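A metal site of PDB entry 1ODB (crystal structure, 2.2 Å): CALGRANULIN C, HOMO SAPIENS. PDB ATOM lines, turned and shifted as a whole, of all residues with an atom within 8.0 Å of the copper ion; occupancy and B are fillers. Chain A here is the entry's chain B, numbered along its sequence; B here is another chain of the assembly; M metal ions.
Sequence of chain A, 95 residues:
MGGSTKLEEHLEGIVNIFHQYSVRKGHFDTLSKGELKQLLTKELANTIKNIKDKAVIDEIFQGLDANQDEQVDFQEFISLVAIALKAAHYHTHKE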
ATOM      1  N   ALA A  88      -7.016  -2.273   6.286  1.00  0.00           N
ATOM      2  CA  ALA A  88      -7.684  -2.011   7.551  1.00  0.00           C
ATOM      3  C   ALA A  88      -6.680  -1.403   8.525  1.00  0.00           C
ATOM      4  O   ALA A  88      -7.028  -0.553   9.364  1.00  0.00           O
ATOM      5  CB  ALA A  88      -8.296  -3.266   8.072  1.00  0.00           C
ATOM      6  N   HIS A  89      -5.414  -1.789   8.383  1.00  0.00           N
ATOM      7  CA  HIS A  89      -4.333  -1.225   9.203  1.00  0.00           C
ATOM      8  C   HIS A  89      -4.052   0.231   8.832  1.00  0.00           C
ATOM      9  O   HIS A  89      -3.796   1.059   9.708  1.00  0.00           O
ATOM     10  CB  HIS A  89      -3.051  -2.057   9.061  1.00  0.00           C
ATOM     11  CG  HIS A  89      -1.950  -1.630   9.997  1.00  0.00           C
ATOM     12  ND1 HIS A  89      -0.621  -1.882   9.739  1.00  0.00           N
ATOM     13  CD2 HIS A  89      -1.987  -0.995  11.185  1.00  0.00           C
ATOM     14  CE1 HIS A  89       0.112  -1.417  10.725  1.00  0.00           C
ATOM     15  NE2 HIS A  89      -0.688  -0.869  11.620  1.00  0.00           N
ATOM     16  N   TYR A  90      -4.104   0.559   7.539  1.00  0.00           N
ATOM     17  CA  TYR A  90      -3.935   1.939   7.076  1.00  0.00           C
ATOM     18  C   TYR A  90      -5.040   2.847   7.625  1.00  0.00           C
ATOM     19  O   TYR A  90      -4.778   3.984   7.975  1.00  0.00           O
ATOM     20  CB  TYR A  90      -3.911   1.995   5.550  1.00  0.00           C
ATOM     21  CG  TYR A  90      -3.784   3.383   4.943  1.00  0.00           C
ATOM     22  CD1 TYR A  90      -2.537   3.998   4.804  1.00  0.00           C
ATOM     23  CD2 TYR A  90      -4.912   4.076   4.473  1.00  0.00           C
ATOM     24  CE1 TYR A  90      -2.412   5.250   4.239  1.00  0.00           C
ATOM     25  CE2 TYR A  90      -4.798   5.328   3.895  1.00  0.00           C
ATOM     26  CZ  TYR A  90      -3.552   5.916   3.789  1.00  0.00           C
ATOM     27  OH  TYR A  90      -3.425   7.154   3.222  1.00  0.00           O
ATOM     28  N   THR A  92      -6.462   2.750  10.539  1.00  0.00           N
ATOM     29  CA  THR A  92      -6.175   3.049  11.943  1.00  0.00           C
ATOM     30  C   THR A  92      -5.071   4.082  12.103  1.00  0.00           C
ATOM     31  O   THR A  92      -4.951   4.705  13.149  1.00  0.00           O
ATOM     32  CB  THR A  92      -5.755   1.776  12.722  1.00  0.00           C
ATOM     33  OG1 THR A  92      -4.440   1.353  12.293  1.00  0.00           O
ATOM     34  CG2 THR A  92      -6.705   0.589  12.440  1.00  0.00           C
ATOM     35  N   HIS A  93      -4.269   4.235  11.063  1.00  0.00           N
ATOM     36  CA  HIS A  93      -3.221   5.253  11.020  1.00  0.00           C
ATOM     37  C   HIS A  93      -3.550   6.441  10.130  1.00  0.00           C
ATOM     38  O   HIS A  93      -2.752   7.360  10.014  1.00  0.00           O
ATOM     39  CB  HIS A  93      -1.910   4.600  10.578  1.00  0.00           C
ATOM     40  CG  HIS A  93      -1.314   3.700  11.612  1.00  0.00           C
ATOM     41  ND1 HIS A  93      -0.562   4.165  12.660  1.00  0.00           N
ATOM     42  CD2 HIS A  93      -1.388   2.357  11.769  1.00  0.00           C
ATOM     43  CE1 HIS A  93      -0.172   3.154  13.404  1.00  0.00           C
ATOM     44  NE2 HIS A  93      -0.667   2.042  12.884  1.00  0.00           N
ATOM     45  N   VAL B  15      -5.804  -7.145  13.074  1.00  0.00           N
ATOM     46  CA  VAL B  15      -4.990  -5.942  13.207  1.00  0.00           C
ATOM     47  C   VAL B  15      -4.829  -5.525  14.661  1.00  0.00           C
ATOM     48  O   VAL B  15      -3.723  -5.221  15.113  1.00  0.00           O
ATOM     49  CB  VAL B  15      -5.611  -4.751  12.429  1.00  0.00           C
ATOM     50  CG1 VAL B  15      -4.893  -3.443  12.734  1.00  0.00           C
ATOM     51  CG2 VAL B  15      -5.545  -5.009  10.965  1.00  0.00           C
ATOM     52  N   ASN B  16      -5.931  -5.503  15.381  1.00  0.00           N
ATOM     53  CA  ASN B  16      -5.892  -5.133  16.784  1.00  0.00           C
ATOM     54  C   ASN B  16      -5.020  -6.082  17.602  1.00  0.00           C
ATOM     55  O   ASN B  16      -4.258  -5.640  18.480  1.00  0.00           O
ATOM     56  CB  ASN B  16      -7.289  -5.037  17.388  1.00  0.00           C
ATOM     57  CG  ASN B  16      -7.242  -4.517  18.815  1.00  0.00           C
ATOM     58  OD1 ASN B  16      -7.336  -5.298  19.751  1.00  0.00           O
ATOM     59  ND2 ASN B  16      -7.056  -3.199  18.991  1.00  0.00           N
ATOM     60  N   PHE B  18      -2.375  -7.837  16.695  1.00  0.00           N
ATOM     61  CA  PHE B  18      -0.967  -7.517  16.466  1.00  0.00           C
ATOM     62  C   PHE B  18      -0.460  -6.403  17.373  1.00  0.00           C
ATOM     63  O   PHE B  18       0.626  -6.486  17.932  1.00  0.00           O
ATOM     64  CB  PHE B  18      -0.764  -7.082  15.001  1.00  0.00           C
ATOM     65  CG  PHE B  18       0.611  -6.568  14.699  1.00  0.00           C
ATOM     66  CD1 PHE B  18       1.627  -7.433  14.307  1.00  0.00           C
ATOM     67  CD2 PHE B  18       0.889  -5.208  14.779  1.00  0.00           C
ATOM     68  CE1 PHE B  18       2.915  -6.928  14.026  1.00  0.00           C
ATOM     69  CE2 PHE B  18       2.149  -4.716  14.508  1.00  0.00           C
ATOM     70  CZ  PHE B  18       3.161  -5.559  14.112  1.00  0.00           C
ATOM     71  N   HIS B  19      -1.257  -5.345  17.516  1.00  0.00           N
ATOM     72  CA  HIS B  19      -0.894  -4.209  18.369  1.00  0.00           C
ATOM     73  C   HIS B  19      -0.892  -4.507  19.854  1.00  0.00           C
ATOM     74  O   HIS B  19      -0.086  -3.952  20.594  1.00  0.00           O
ATOM     75  CB  HIS B  19      -1.797  -3.015  18.070  1.00  0.00           C
ATOM     76  CG  HIS B  19      -1.620  -2.476  16.701  1.00  0.00           C
ATOM     77  ND1 HIS B  19      -2.242  -3.022  15.601  1.00  0.00           N
ATOM     78  CD2 HIS B  19      -0.859  -1.446  16.237  1.00  0.00           C
ATOM     79  CE1 HIS B  19      -1.883  -2.353  14.522  1.00  0.00           C
ATOM     80  NE2 HIS B  19      -1.045  -1.403  14.872  1.00  0.00           N
ATOM     81  N   SER B  22       2.548  -5.974  20.017  1.00  0.00           N
ATOM     82  CA  SER B  22       3.635  -5.160  19.488  1.00  0.00           C
ATOM     83  C   SER B  22       4.029  -3.961  20.345  1.00  0.00           C
ATOM     84  O   SER B  22       5.187  -3.486  20.276  1.00  0.00           O
ATOM     85  CB  SER B  22       3.353  -4.680  18.056  1.00  0.00           C
ATOM     86  OG  SER B  22       2.368  -3.644  18.003  1.00  0.00           O
ATOM     87  N   VAL B  23       3.101  -3.501  21.171  1.00  0.00           N
ATOM     88  CA  VAL B  23       3.355  -2.351  22.065  1.00  0.00           C
ATOM     89  C   VAL B  23       4.112  -2.730  23.354  1.00  0.00           C
ATOM     90  O   VAL B  23       4.510  -1.841  24.158  1.00  0.00           O
ATOM     91  CB  VAL B  23       2.046  -1.633  22.457  1.00  0.00           C
ATOM     92  CG1 VAL B  23       1.292  -1.134  21.190  1.00  0.00           C
ATOM     93  CG2 VAL B  23       1.128  -2.521  23.368  1.00  0.00           C
ATOM     94  N   PHE B  28       6.983   0.073  19.120  1.00  0.00           N
ATOM     95  CA  PHE B  28       5.557  -0.161  19.334  1.00  0.00           C
ATOM     96  C   PHE B  28       4.889  -0.702  18.055  1.00  0.00           C
ATOM     97  O   PHE B  28       3.812  -1.231  18.126  1.00  0.00           O
ATOM     98  CB  PHE B  28       4.873   1.116  19.825  1.00  0.00           C
ATOM     99  CG  PHE B  28       5.399   1.629  21.153  1.00  0.00           C
ATOM    100  CD1 PHE B  28       5.078   0.988  22.323  1.00  0.00           C
ATOM    101  CD2 PHE B  28       6.241   2.725  21.204  1.00  0.00           C
ATOM    102  CE1 PHE B  28       5.568   1.446  23.542  1.00  0.00           C
ATOM    103  CE2 PHE B  28       6.752   3.179  22.426  1.00  0.00           C
ATOM    104  CZ  PHE B  28       6.412   2.529  23.590  1.00  0.00           C
ATOM    105  N   ASP B  29       5.566  -0.561  16.910  1.00  0.00           N
ATOM    106  CA  ASP B  29       5.039  -0.991  15.607  1.00  0.00           C
ATOM    107  C   ASP B  29       5.516  -2.398  15.155  1.00  0.00           C
ATOM    108  O   ASP B  29       5.144  -2.837  14.072  1.00  0.00           O
ATOM    109  CB  ASP B  29       5.307   0.067  14.497  1.00  0.00           C
ATOM    110  CG  ASP B  29       6.794   0.324  14.240  1.00  0.00           C
ATOM    111  OD1 ASP B  29       7.628   0.137  15.144  1.00  0.00           O
ATOM    112  OD2 ASP B  29       7.220   0.767  13.144  1.00  0.00           O
ATOM    113  N   PHE B  74       4.359  -5.353  10.526  1.00  0.00           N
ATOM    114  CA  PHE B  74       2.975  -5.745  10.331  1.00  0.00           C
ATOM    115  C   PHE B  74       2.843  -6.608   9.042  1.00  0.00           C
ATOM    116  O   PHE B  74       2.147  -7.584   9.011  1.00  0.00           O
ATOM    117  CB  PHE B  74       2.026  -4.546  10.292  1.00  0.00           C
ATOM    118  CG  PHE B  74       0.574  -4.967  10.083  1.00  0.00           C
ATOM    119  CD1 PHE B  74      -0.155  -5.497  11.109  1.00  0.00           C
ATOM    120  CD2 PHE B  74      -0.004  -4.891   8.822  1.00  0.00           C
ATOM    121  CE1 PHE B  74      -1.452  -5.930  10.895  1.00  0.00           C
ATOM    122  CE2 PHE B  74      -1.293  -5.314   8.601  1.00  0.00           C
ATOM    123  CZ  PHE B  74      -2.017  -5.848   9.654  1.00  0.00           C
HETATM  124 CU    CU M   1      -0.665   0.241  13.679  1.00  0.00          CU
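O of Val 15 of chain B lies within hydrogen-bond range of ND1 of His 19 of chain B, at 2.7 Å.
The side-chain hydroxyl (OG1) of Thr 92 sits at hydrogen-bond distance from the backbone carbonyl oxygen (O) of His 89 (2.7 Å).
The nearest printed residue that does not touch the copper ion is Thr 92 (4.2 Å).
The copper ion is bound by NE2 of His 93, NE2 of His 19 of chain B and NE2 of His 89.
The copper ion has three donor atoms within binding distance.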
